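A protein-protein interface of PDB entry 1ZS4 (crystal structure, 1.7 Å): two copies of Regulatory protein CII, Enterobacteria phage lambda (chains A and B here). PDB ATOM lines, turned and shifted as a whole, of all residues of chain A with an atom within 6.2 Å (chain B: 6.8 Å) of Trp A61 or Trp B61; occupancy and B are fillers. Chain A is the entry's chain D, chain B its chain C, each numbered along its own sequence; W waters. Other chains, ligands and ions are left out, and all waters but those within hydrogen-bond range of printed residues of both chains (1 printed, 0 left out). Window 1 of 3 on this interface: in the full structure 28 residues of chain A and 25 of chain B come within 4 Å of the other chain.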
ATOM      1  N   GLU A  10      -1.166  23.393  28.880  1.00  0.00           N
ATOM      2  CA  GLU A  10      -2.421  23.421  28.127  1.00  0.00           C
ATOM      3  C   GLU A  10      -3.239  22.128  28.107  1.00  0.00           C
ATOM      4  O   GLU A  10      -4.470  22.165  28.248  1.00  0.00           O
ATOM      5  CB  GLU A  10      -2.151  23.894  26.697  1.00  0.00           C
ATOM      6  CG  GLU A  10      -3.414  24.200  25.901  1.00  0.00           C
ATOM      7  CD  GLU A  10      -4.170  25.433  26.405  1.00  0.00           C
ATOM      8  OE1 GLU A  10      -5.211  25.773  25.797  1.00  0.00           O
ATOM      9  OE2 GLU A  10      -3.732  26.065  27.396  1.00  0.00           O
ATOM     10  N   ARG A  13      -5.050  21.775  31.262  1.00  0.00           N
ATOM     11  CA  ARG A  13      -6.121  22.769  31.343  1.00  0.00           C
ATOM     12  C   ARG A  13      -7.316  22.237  30.557  1.00  0.00           C
ATOM     13  O   ARG A  13      -8.464  22.241  31.037  1.00  0.00           O
ATOM     14  CB  ARG A  13      -5.636  24.100  30.762  1.00  0.00           C
ATOM     15  CG  ARG A  13      -6.687  25.195  30.702  1.00  0.00           C
ATOM     16  CD  ARG A  13      -6.061  26.493  30.186  1.00  0.00           C
ATOM     17  NE  ARG A  13      -7.041  27.565  30.045  1.00  0.00           N
ATOM     18  CZ  ARG A  13      -7.921  27.652  29.053  1.00  0.00           C
ATOM     19  NH1 ARG A  13      -7.947  26.726  28.098  1.00  0.00           N
ATOM     20  NH2 ARG A  13      -8.777  28.669  29.017  1.00  0.00           N
ATOM     21  N   ILE A  14      -7.039  21.775  29.343  1.00  0.00           N
ATOM     22  CA  ILE A  14      -8.092  21.218  28.488  1.00  0.00           C
ATOM     23  C   ILE A  14      -8.739  19.986  29.154  1.00  0.00           C
ATOM     24  O   ILE A  14      -9.972  19.868  29.236  1.00  0.00           O
ATOM     25  CB  ILE A  14      -7.507  20.822  27.095  1.00  0.00           C
ATOM     26  CG1 ILE A  14      -7.173  22.090  26.299  1.00  0.00           C
ATOM     27  CG2 ILE A  14      -8.485  19.916  26.345  1.00  0.00           C
ATOM     28  CD1 ILE A  14      -6.496  21.842  24.949  1.00  0.00           C
ATOM     29  N   GLU A  15      -7.921  19.071  29.654  1.00  0.00           N
ATOM     30  CA  GLU A  15      -8.485  17.878  30.284  1.00  0.00           C
ATOM     31  C   GLU A  15      -9.403  18.183  31.464  1.00  0.00           C
ATOM     32  O   GLU A  15     -10.460  17.557  31.620  1.00  0.00           O
ATOM     33  CB  GLU A  15      -7.371  16.936  30.753  1.00  0.00           C
ATOM     34  CG  GLU A  15      -7.934  15.680  31.420  1.00  0.00           C
ATOM     35  CD  GLU A  15      -6.865  14.642  31.717  1.00  0.00           C
ATOM     36  OE1 GLU A  15      -6.438  14.526  32.886  1.00  0.00           O
ATOM     37  OE2 GLU A  15      -6.458  13.942  30.768  1.00  0.00           O
ATOM     38  N   ALA A  17     -11.176  20.957  32.101  1.00  0.00           N
ATOM     39  CA  ALA A  17     -12.419  21.529  31.612  1.00  0.00           C
ATOM     40  C   ALA A  17     -13.257  20.478  30.907  1.00  0.00           C
ATOM     41  O   ALA A  17     -14.476  20.456  31.048  1.00  0.00           O
ATOM     42  CB  ALA A  17     -12.133  22.665  30.667  1.00  0.00           C
ATOM     43  N   LEU A  18     -12.601  19.610  30.146  1.00  0.00           N
ATOM     44  CA  LEU A  18     -13.304  18.575  29.404  1.00  0.00           C
ATOM     45  C   LEU A  18     -13.975  17.565  30.348  1.00  0.00           C
ATOM     46  O   LEU A  18     -15.172  17.285  30.225  1.00  0.00           O
ATOM     47  CB  LEU A  18     -12.319  17.885  28.443  1.00  0.00           C
ATOM     48  CG  LEU A  18     -12.821  16.853  27.422  1.00  0.00           C
ATOM     49  CD1 LEU A  18     -14.098  17.353  26.751  1.00  0.00           C
ATOM     50  CD2 LEU A  18     -11.738  16.596  26.369  1.00  0.00           C
ATOM     51  N   LEU A  19     -13.223  17.036  31.311  1.00  0.00           N
ATOM     52  CA  LEU A  19     -13.796  16.073  32.225  1.00  0.00           C
ATOM     53  C   LEU A  19     -14.912  16.693  33.061  1.00  0.00           C
ATOM     54  O   LEU A  19     -15.892  16.017  33.378  1.00  0.00           O
ATOM     55  CB  LEU A  19     -12.714  15.475  33.112  1.00  0.00           C
ATOM     56  CG  LEU A  19     -11.713  14.585  32.390  1.00  0.00           C
ATOM     57  CD1 LEU A  19     -10.550  14.224  33.303  1.00  0.00           C
ATOM     58  CD2 LEU A  19     -12.388  13.334  31.867  1.00  0.00           C
ATOM     59  N   LYS A  21     -16.962  19.105  32.113  1.00  0.00           N
ATOM     60  CA  LYS A  21     -18.161  19.264  31.289  1.00  0.00           C
ATOM     61  C   LYS A  21     -18.788  17.880  31.067  1.00  0.00           C
ATOM     62  O   LYS A  21     -20.019  17.732  30.987  1.00  0.00           O
ATOM     63  CB  LYS A  21     -17.812  19.914  29.939  1.00  0.00           C
ATOM     64  CG  LYS A  21     -18.988  20.585  29.240  1.00  0.00           C
ATOM     65  CD  LYS A  21     -19.537  21.737  30.098  1.00  0.00           C
ATOM     66  CE  LYS A  21     -20.735  22.431  29.463  1.00  0.00           C
ATOM     67  NZ  LYS A  21     -20.391  23.147  28.199  1.00  0.00           N
ATOM     68  N   LEU A  55      -4.144  15.868  22.132  1.00  0.00           N
ATOM     69  CA  LEU A  55      -4.393  16.158  20.725  1.00  0.00           C
ATOM     70  C   LEU A  55      -4.971  17.577  20.584  1.00  0.00           C
ATOM     71  O   LEU A  55      -4.506  18.348  19.739  1.00  0.00           O
ATOM     72  CB  LEU A  55      -5.364  15.144  20.105  1.00  0.00           C
ATOM     73  CG  LEU A  55      -5.702  15.429  18.624  1.00  0.00           C
ATOM     74  CD1 LEU A  55      -4.463  15.293  17.717  1.00  0.00           C
ATOM     75  CD2 LEU A  55      -6.746  14.449  18.195  1.00  0.00           C
ATOM     76  N   LEU A  56      -5.969  17.928  21.403  1.00  0.00           N
ATOM     77  CA  LEU A  56      -6.564  19.273  21.333  1.00  0.00           C
ATOM     78  C   LEU A  56      -5.557  20.374  21.645  1.00  0.00           C
ATOM     79  O   LEU A  56      -5.585  21.441  21.016  1.00  0.00           O
ATOM     80  CB  LEU A  56      -7.794  19.403  22.252  1.00  0.00           C
ATOM     81  CG  LEU A  56      -8.990  18.520  21.858  1.00  0.00           C
ATOM     82  CD1 LEU A  56     -10.146  18.810  22.823  1.00  0.00           C
ATOM     83  CD2 LEU A  56      -9.429  18.766  20.402  1.00  0.00           C
ATOM     84  N   ALA A  57      -4.663  20.121  22.596  1.00  0.00           N
ATOM     85  CA  ALA A  57      -3.626  21.104  22.939  1.00  0.00           C
ATOM     86  C   ALA A  57      -2.739  21.331  21.710  1.00  0.00           C
ATOM     87  O   ALA A  57      -2.419  22.472  21.335  1.00  0.00           O
ATOM     88  CB  ALA A  57      -2.787  20.588  24.093  1.00  0.00           C
ATOM     89  N   VAL A  58      -2.345  20.229  21.079  1.00  0.00           N
ATOM     90  CA  VAL A  58      -1.495  20.272  19.897  1.00  0.00           C
ATOM     91  C   VAL A  58      -2.160  20.997  18.738  1.00  0.00           C
ATOM     92  O   VAL A  58      -1.505  21.729  17.995  1.00  0.00           O
ATOM     93  CB  VAL A  58      -1.119  18.844  19.460  1.00  0.00           C
ATOM     94  CG1 VAL A  58      -0.589  18.831  18.015  1.00  0.00           C
ATOM     95  CG2 VAL A  58      -0.058  18.301  20.422  1.00  0.00           C
ATOM     96  N   LEU A  59      -3.459  20.793  18.575  1.00  0.00           N
ATOM     97  CA  LEU A  59      -4.177  21.448  17.494  1.00  0.00           C
ATOM     98  C   LEU A  59      -4.608  22.857  17.878  1.00  0.00           C
ATOM     99  O   LEU A  59      -5.341  23.524  17.140  1.00  0.00           O
ATOM    100  CB  LEU A  59      -5.395  20.621  17.110  1.00  0.00           C
ATOM    101  CG  LEU A  59      -5.094  19.187  16.654  1.00  0.00           C
ATOM    102  CD1 LEU A  59      -6.397  18.484  16.330  1.00  0.00           C
ATOM    103  CD2 LEU A  59      -4.175  19.223  15.455  1.00  0.00           C
ATOM    104  N   GLU A  60      -4.156  23.294  19.046  1.00  0.00           N
ATOM    105  CA  GLU A  60      -4.454  24.631  19.553  1.00  0.00           C
ATOM    106  C   GLU A  60      -5.943  24.922  19.650  1.00  0.00           C
ATOM    107  O   GLU A  60      -6.406  26.028  19.373  1.00  0.00           O
ATOM    108  CB  GLU A  60      -3.723  25.671  18.682  1.00  0.00           C
ATOM    109  CG  GLU A  60      -2.195  25.581  18.874  1.00  0.00           C
ATOM    110  CD  GLU A  60      -1.409  26.660  18.141  1.00  0.00           C
ATOM    111  OE1 GLU A  60      -1.885  27.814  18.097  1.00  0.00           O
ATOM    112  OE2 GLU A  60      -0.300  26.359  17.632  1.00  0.00           O
ATOM    113  N   TRP A  61      -6.702  23.915  20.073  1.00  0.00           N
ATOM    114  CA  TRP A  61      -8.146  24.062  20.219  1.00  0.00           C
ATOM    115  C   TRP A  61      -8.462  25.159  21.247  1.00  0.00           C
ATOM    116  O   TRP A  61      -7.985  25.107  22.383  1.00  0.00           O
ATOM    117  CB  TRP A  61      -8.738  22.732  20.677  1.00  0.00           C
ATOM    118  CG  TRP A  61     -10.210  22.552  20.398  1.00  0.00           C
ATOM    119  CD1 TRP A  61     -11.235  22.657  21.298  1.00  0.00           C
ATOM    120  CD2 TRP A  61     -10.794  22.145  19.164  1.00  0.00           C
ATOM    121  NE1 TRP A  61     -12.431  22.327  20.695  1.00  0.00           N
ATOM    122  CE2 TRP A  61     -12.185  22.011  19.381  1.00  0.00           C
ATOM    123  CE3 TRP A  61     -10.273  21.871  17.886  1.00  0.00           C
ATOM    124  CZ2 TRP A  61     -13.069  21.611  18.367  1.00  0.00           C
ATOM    125  CZ3 TRP A  61     -11.152  21.473  16.871  1.00  0.00           C
ATOM    126  CH2 TRP A  61     -12.543  21.346  17.123  1.00  0.00           C
ATOM    127  N   GLY A  62      -9.258  26.149  20.836  1.00  0.00           N
ATOM    128  CA  GLY A  62      -9.619  27.232  21.739  1.00  0.00           C
ATOM    129  C   GLY A  62      -8.724  28.455  21.658  1.00  0.00           C
ATOM    130  O   GLY A  62      -9.122  29.550  22.095  1.00  0.00           O
ATOM    131  N   VAL A  63      -7.522  28.272  21.108  1.00  0.00           N
ATOM    132  CA  VAL A  63      -6.539  29.348  20.972  1.00  0.00           C
ATOM    133  C   VAL A  63      -7.027  30.413  19.999  1.00  0.00           C
ATOM    134  O   VAL A  63      -6.943  31.609  20.281  1.00  0.00           O
ATOM    135  CB  VAL A  63      -5.167  28.807  20.476  1.00  0.00           C
ATOM    136  CG1 VAL A  63      -4.208  29.970  20.170  1.00  0.00           C
ATOM    137  CG2 VAL A  63      -4.550  27.906  21.541  1.00  0.00           C
ATOM    138  N   VAL A  64      -7.549  29.990  18.853  1.00  0.00           N
ATOM    139  CA  VAL A  64      -8.035  30.964  17.889  1.00  0.00           C
ATOM    140  C   VAL A  64      -9.188  31.784  18.494  1.00  0.00           C
ATOM    141  O   VAL A  64      -9.253  33.005  18.309  1.00  0.00           O
ATOM    142  CB  VAL A  64      -8.480  30.263  16.598  1.00  0.00           C
ATOM    143  CG1 VAL A  64      -8.888  31.288  15.554  1.00  0.00           C
ATOM    144  CG2 VAL A  64      -7.336  29.405  16.085  1.00  0.00           C
ATOM    145  N   GLU B  10     -23.402  20.258  14.052  1.00  0.00           N
ATOM    146  CA  GLU B  10     -22.259  20.760  14.810  1.00  0.00           C
ATOM    147  C   GLU B  10     -21.208  19.658  14.953  1.00  0.00           C
ATOM    148  O   GLU B  10     -20.011  19.940  14.931  1.00  0.00           O
ATOM    149  CB  GLU B  10     -22.701  21.263  16.192  1.00  0.00           C
ATOM    150  CG  GLU B  10     -21.569  21.842  17.050  1.00  0.00           C
ATOM    151  CD  GLU B  10     -20.911  23.094  16.466  1.00  0.00           C
ATOM    152  OE1 GLU B  10     -21.315  23.567  15.375  1.00  0.00           O
ATOM    153  OE2 GLU B  10     -19.971  23.622  17.120  1.00  0.00           O
ATOM    154  N   ARG B  13     -19.348  19.611  11.779  1.00  0.00           N
ATOM    155  CA  ARG B  13     -18.486  20.788  11.668  1.00  0.00           C
ATOM    156  C   ARG B  13     -17.221  20.569  12.495  1.00  0.00           C
ATOM    157  O   ARG B  13     -16.111  20.833  12.033  1.00  0.00           O
ATOM    158  CB  ARG B  13     -19.208  22.038  12.184  1.00  0.00           C
ATOM    159  CG  ARG B  13     -18.469  23.344  11.898  1.00  0.00           C
ATOM    160  CD  ARG B  13     -19.259  24.535  12.399  1.00  0.00           C
ATOM    161  NE  ARG B  13     -19.192  24.668  13.855  1.00  0.00           N
ATOM    162  CZ  ARG B  13     -18.188  25.245  14.510  1.00  0.00           C
ATOM    163  NH1 ARG B  13     -17.158  25.752  13.844  1.00  0.00           N
ATOM    164  NH2 ARG B  13     -18.220  25.317  15.838  1.00  0.00           N
ATOM    165  N   ILE B  14     -17.393  20.092  13.727  1.00  0.00           N
ATOM    166  CA  ILE B  14     -16.246  19.836  14.600  1.00  0.00           C
ATOM    167  C   ILE B  14     -15.332  18.756  14.025  1.00  0.00           C
ATOM    168  O   ILE B  14     -14.104  18.885  14.073  1.00  0.00           O
ATOM    169  CB  ILE B  14     -16.706  19.425  16.019  1.00  0.00           C
ATOM    170  CG1 ILE B  14     -17.329  20.642  16.715  1.00  0.00           C
ATOM    171  CG2 ILE B  14     -15.508  18.896  16.854  1.00  0.00           C
ATOM    172  CD1 ILE B  14     -18.039  20.298  18.031  1.00  0.00           C
ATOM    173  N   GLU B  15     -15.918  17.690  13.486  1.00  0.00           N
ATOM    174  CA  GLU B  15     -15.122  16.613  12.895  1.00  0.00           C
ATOM    175  C   GLU B  15     -14.271  17.142  11.737  1.00  0.00           C
ATOM    176  O   GLU B  15     -13.081  16.837  11.619  1.00  0.00           O
ATOM    177  CB  GLU B  15     -16.037  15.502  12.362  1.00  0.00           C
ATOM    178  CG  GLU B  15     -15.257  14.312  11.795  1.00  0.00           C
ATOM    179  CD  GLU B  15     -16.166  13.250  11.204  1.00  0.00           C
ATOM    180  OE1 GLU B  15     -17.374  13.265  11.516  1.00  0.00           O
ATOM    181  OE2 GLU B  15     -15.666  12.395  10.439  1.00  0.00           O
ATOM    182  N   ALA B  17     -13.323  20.152  11.291  1.00  0.00           N
ATOM    183  CA  ALA B  17     -12.326  21.061  11.856  1.00  0.00           C
ATOM    184  C   ALA B  17     -11.133  20.281  12.388  1.00  0.00           C
ATOM    185  O   ALA B  17      -9.984  20.651  12.153  1.00  0.00           O
ATOM    186  CB  ALA B  17     -12.948  21.890  12.982  1.00  0.00           C
ATOM    187  N   LEU B  18     -11.410  19.208  13.128  1.00  0.00           N
ATOM    188  CA  LEU B  18     -10.345  18.389  13.682  1.00  0.00           C
ATOM    189  C   LEU B  18      -9.514  17.748  12.572  1.00  0.00           C
ATOM    190  O   LEU B  18      -8.289  17.803  12.604  1.00  0.00           O
ATOM    191  CB  LEU B  18     -10.920  17.297  14.588  1.00  0.00           C
ATOM    192  CG  LEU B  18     -11.390  17.790  15.962  1.00  0.00           C
ATOM    193  CD1 LEU B  18     -12.160  16.681  16.662  1.00  0.00           C
ATOM    194  CD2 LEU B  18     -10.206  18.253  16.808  1.00  0.00           C
ATOM    195  N   LYS B  21      -7.438  20.360  10.793  1.00  0.00           N
ATOM    196  CA  LYS B  21      -6.303  20.820  11.603  1.00  0.00           C
ATOM    197  C   LYS B  21      -5.172  19.789  11.628  1.00  0.00           C
ATOM    198  O   LYS B  21      -3.986  20.139  11.554  1.00  0.00           O
ATOM    199  CB  LYS B  21      -6.764  21.145  13.036  1.00  0.00           C
ATOM    200  CG  LYS B  21      -7.609  22.417  13.105  1.00  0.00           C
ATOM    201  CD  LYS B  21      -8.209  22.623  14.494  1.00  0.00           C
ATOM    202  CE  LYS B  21      -9.326  23.683  14.482  1.00  0.00           C
ATOM    203  NZ  LYS B  21      -8.791  25.031  14.100  1.00  0.00           N
ATOM    204  N   PHE B  52     -15.909  11.273  18.873  1.00  0.00           N
ATOM    205  CA  PHE B  52     -15.469  12.288  19.819  1.00  0.00           C
ATOM    206  C   PHE B  52     -16.037  13.650  19.405  1.00  0.00           C
ATOM    207  O   PHE B  52     -16.354  14.471  20.263  1.00  0.00           O
ATOM    208  CB  PHE B  52     -13.939  12.326  19.875  1.00  0.00           C
ATOM    209  CG  PHE B  52     -13.384  13.323  20.863  1.00  0.00           C
ATOM    210  CD1 PHE B  52     -13.650  13.209  22.225  1.00  0.00           C
ATOM    211  CD2 PHE B  52     -12.558  14.356  20.426  1.00  0.00           C
ATOM    212  CE1 PHE B  52     -13.102  14.106  23.151  1.00  0.00           C
ATOM    213  CE2 PHE B  52     -11.993  15.268  21.347  1.00  0.00           C
ATOM    214  CZ  PHE B  52     -12.269  15.141  22.712  1.00  0.00           C
ATOM    215  N   LEU B  55     -19.426  14.032  20.784  1.00  0.00           N
ATOM    216  CA  LEU B  55     -19.341  14.372  22.210  1.00  0.00           C
ATOM    217  C   LEU B  55     -19.009  15.881  22.355  1.00  0.00           C
ATOM    218  O   LEU B  55     -19.638  16.601  23.136  1.00  0.00           O
ATOM    219  CB  LEU B  55     -18.251  13.540  22.910  1.00  0.00           C
ATOM    220  CG  LEU B  55     -18.027  13.914  24.383  1.00  0.00           C
ATOM    221  CD1 LEU B  55     -19.324  13.707  25.167  1.00  0.00           C
ATOM    222  CD2 LEU B  55     -16.892  13.051  24.986  1.00  0.00           C
ATOM    223  N   LEU B  56     -18.028  16.367  21.604  1.00  0.00           N
ATOM    224  CA  LEU B  56     -17.684  17.781  21.712  1.00  0.00           C
ATOM    225  C   LEU B  56     -18.882  18.657  21.338  1.00  0.00           C
ATOM    226  O   LEU B  56     -19.072  19.721  21.908  1.00  0.00           O
ATOM    227  CB  LEU B  56     -16.472  18.121  20.835  1.00  0.00           C
ATOM    228  CG  LEU B  56     -15.127  17.529  21.277  1.00  0.00           C
ATOM    229  CD1 LEU B  56     -14.021  18.193  20.439  1.00  0.00           C
ATOM    230  CD2 LEU B  56     -14.863  17.784  22.756  1.00  0.00           C
ATOM    231  N   ALA B  57     -19.691  18.206  20.380  1.00  0.00           N
ATOM    232  CA  ALA B  57     -20.867  18.983  19.976  1.00  0.00           C
ATOM    233  C   ALA B  57     -21.867  19.071  21.136  1.00  0.00           C
ATOM    234  O   ALA B  57     -22.413  20.148  21.434  1.00  0.00           O
ATOM    235  CB  ALA B  57     -21.530  18.349  18.757  1.00  0.00           C
ATOM    236  N   VAL B  58     -22.101  17.938  21.789  1.00  0.00           N
ATOM    237  CA  VAL B  58     -23.016  17.892  22.916  1.00  0.00           C
ATOM    238  C   VAL B  58     -22.509  18.759  24.064  1.00  0.00           C
ATOM    239  O   VAL B  58     -23.300  19.368  24.787  1.00  0.00           O
ATOM    240  CB  VAL B  58     -23.215  16.441  23.375  1.00  0.00           C
ATOM    241  CG1 VAL B  58     -23.961  16.401  24.714  1.00  0.00           C
ATOM    242  CG2 VAL B  58     -23.984  15.696  22.306  1.00  0.00           C
ATOM    243  N   LEU B  59     -21.190  18.845  24.211  1.00  0.00           N
ATOM    244  CA  LEU B  59     -20.569  19.655  25.261  1.00  0.00           C
ATOM    245  C   LEU B  59     -20.449  21.129  24.891  1.00  0.00           C
ATOM    246  O   LEU B  59     -20.047  21.951  25.727  1.00  0.00           O
ATOM    247  CB  LEU B  59     -19.164  19.114  25.566  1.00  0.00           C
ATOM    248  CG  LEU B  59     -19.065  17.674  26.061  1.00  0.00           C
ATOM    249  CD1 LEU B  59     -17.592  17.292  26.243  1.00  0.00           C
ATOM    250  CD2 LEU B  59     -19.815  17.549  27.363  1.00  0.00           C
ATOM    251  N   GLU B  60     -20.812  21.460  23.648  1.00  0.00           N
ATOM    252  CA  GLU B  60     -20.715  22.821  23.119  1.00  0.00           C
ATOM    253  C   GLU B  60     -19.255  23.281  23.089  1.00  0.00           C
ATOM    254  O   GLU B  60     -18.931  24.426  23.430  1.00  0.00           O
ATOM    255  CB  GLU B  60     -21.576  23.778  23.954  1.00  0.00           C
ATOM    256  CG  GLU B  60     -23.056  23.627  23.666  1.00  0.00           C
ATOM    257  CD  GLU B  60     -23.906  24.512  24.558  1.00  0.00           C
ATOM    258  OE1 GLU B  60     -23.558  25.702  24.706  1.00  0.00           O
ATOM    259  OE2 GLU B  60     -24.918  24.020  25.109  1.00  0.00           O
ATOM    260  N   TRP B  61     -18.385  22.364  22.666  1.00  0.00           N
ATOM    261  CA  TRP B  61     -16.951  22.598  22.578  1.00  0.00           C
ATOM    262  C   TRP B  61     -16.421  22.893  21.172  1.00  0.00           C
ATOM    263  O   TRP B  61     -15.225  22.764  20.897  1.00  0.00           O
ATOM    264  CB  TRP B  61     -16.195  21.408  23.183  1.00  0.00           C
ATOM    265  CG  TRP B  61     -15.806  21.646  24.602  1.00  0.00           C
ATOM    266  CD1 TRP B  61     -16.599  22.138  25.603  1.00  0.00           C
ATOM    267  CD2 TRP B  61     -14.519  21.430  25.177  1.00  0.00           C
ATOM    268  NE1 TRP B  61     -15.876  22.245  26.769  1.00  0.00           N
ATOM    269  CE2 TRP B  61     -14.596  21.817  26.535  1.00  0.00           C
ATOM    270  CE3 TRP B  61     -13.303  20.949  24.675  1.00  0.00           C
ATOM    271  CZ2 TRP B  61     -13.502  21.736  27.400  1.00  0.00           C
ATOM    272  CZ3 TRP B  61     -12.213  20.870  25.535  1.00  0.00           C
ATOM    273  CH2 TRP B  61     -12.323  21.263  26.885  1.00  0.00           C
ATOM    274  N   GLY B  62     -17.302  23.295  20.272  1.00  0.00           N
ATOM    275  CA  GLY B  62     -16.825  23.636  18.944  1.00  0.00           C
ATOM    276  C   GLY B  62     -16.053  24.951  19.007  1.00  0.00           C
ATOM    277  O   GLY B  62     -16.206  25.741  19.959  1.00  0.00           O
ATOM    278  N   VAL B  63     -15.219  25.198  18.004  1.00  0.00           N
ATOM    279  CA  VAL B  63     -14.433  26.421  17.964  1.00  0.00           C
ATOM    280  C   VAL B  63     -14.676  27.202  16.679  1.00  0.00           C
ATOM    281  O   VAL B  63     -15.255  26.688  15.717  1.00  0.00           O
ATOM    282  CB  VAL B  63     -12.919  26.123  18.125  1.00  0.00           C
ATOM    283  CG1 VAL B  63     -12.667  25.533  19.501  1.00  0.00           C
ATOM    284  CG2 VAL B  63     -12.452  25.136  17.053  1.00  0.00           C
HETATM  285  O   HOH W   1      -6.942  25.743  16.179  1.00  0.00           O
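Water W1 lies within hydrogen-bond range of NZ of Lys B21 (2.9 Å), O of Leu A59 (2.9 Å) and O of Glu A60 (3.3 Å).
Of the 18 printed residues of chain A, 8 touch a printed residue of chain B.
Printed residues of chain A that touch a printed residue of chain B: Ile A14, Ala A17, Leu A18, Lys A21, Leu A56, Leu A59, Trp A61 and Gly A62.
Hydrophobic or aromatic side chains of chain A within 4 Å of the printed part of chain B: Ile A14, Ala A17, Leu A18, Leu A56, Leu A59 and Trp A61.
Of the 17 printed residues of chain B, 7 touch a printed residue of chain A.
Hydrophobic or aromatic side chains of chain B that line the printed part of chain A: Ile B14, Leu B18, Phe B52, Leu B59, Trp B61 and Val B63.
The guanidinium group of Arg B13 lies within hydrogen-bond range of the backbone carbonyl oxygen of Val B63 (2.8 Å).
The backbone carbonyl oxygen (O) of Leu B56 is in hydrogen-bond range of the backbone NH (N) of Trp B61, at 2.8 Å.
The backbone carbonyl oxygen (O) of Leu A56 sits at hydrogen-bond distance from the backbone NH (N) of Trp A61 (2.9 Å).
Leu A18 touches Leu B59, and with the chains exchanged Leu A59 touches Leu B18.
Lys A21 touches Leu B59, and with the chains exchanged Leu A59 touches Lys B21.
Leu A56 touches Trp B61, but with the chains exchanged Trp A61 does not touch Leu B56 (4.1 Å).
Trp A61 touches Val B63, but with the chains exchanged Val A63 does not touch Trp B61 (9.5 Å).
Positions printed for both chains: 10, 13, 14, 15, 17, 18, 21, 55, 56, 57, 58, 59, 60, 61, 62 and 63.
Of the 16 pairs that touch across the chains among the printed residues, 9 have their exchanged pair printed and touching as well.
Printed residues of chain B within 4 Å of Trp A61: Ile B14 (3.9 Å), Leu B18 (3.4 Å), Lys B21 (3.7 Å), Trp B61 (2.8 Å) and Val B63 (3.4 Å).
Of the printed residues of chain A, Trp B61 touches Ile A14, Ala A17, Leu A18, Leu A56 and Trp A61.
Of the printed residues of chain B, Lys A21 touches Leu B59 (2.8 Å).
Of the printed residues of chain B, Leu A56 touches Leu B18 (3.7 Å) and Trp B61 (3.98 Å).
Printed residues of chain A within 4 Å of Val B63: Trp A61 (3.4 Å) and Gly A62 (3.7 Å).
Of the printed residues of chain A, Leu B18 touches Leu A56, Leu A59 and Trp A61.
Of the printed residues of chain A, Lys B21 touches Leu A59 and Trp A61.
The nearest residue of chain B that does not touch Trp A61 is Leu B56 (4.1 Å).
The nearest printed residue of chain A that does not touch Trp B61 is Lys A21 (4.3 Å).
The nearest printed residue of chain B that does not touch Ile A14 is Phe B52 (7.1 Å).
Among the printed residues, pairs that only touch across the chains: Ile A14 with Trp B61 (3.6 Å), Ala A17 with Trp B61 (3.7 Å), Leu A18 with Phe B52 (3.97 Å), Leu A18 with Leu B59 (3.5 Å), Leu A18 with Trp B61 (3.6 Å), Leu A56 with Leu B18 (3.7 Å), Leu A56 with Trp B61 (3.98 Å), Leu A59 with Leu B18 (3.8 Å), Leu A59 with Lys B21 (3.995 Å), Trp A61 with Ile B14 (3.9 Å), Trp A61 with Leu B18 (3.4 Å), Trp A61 with Lys B21 (3.7 Å), Trp A61 with Val B63 (3.4 Å) and Gly A62 with Val B63 (3.7 Å).
NZ of Lys A21 lies within hydrogen-bond range of O of Leu B59 (2.8 Å).
The backbone carbonyl oxygen (O) of Trp B61 sits at hydrogen-bond distance from the indole nitrogen (NE1) of Trp A61 (2.8 Å).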
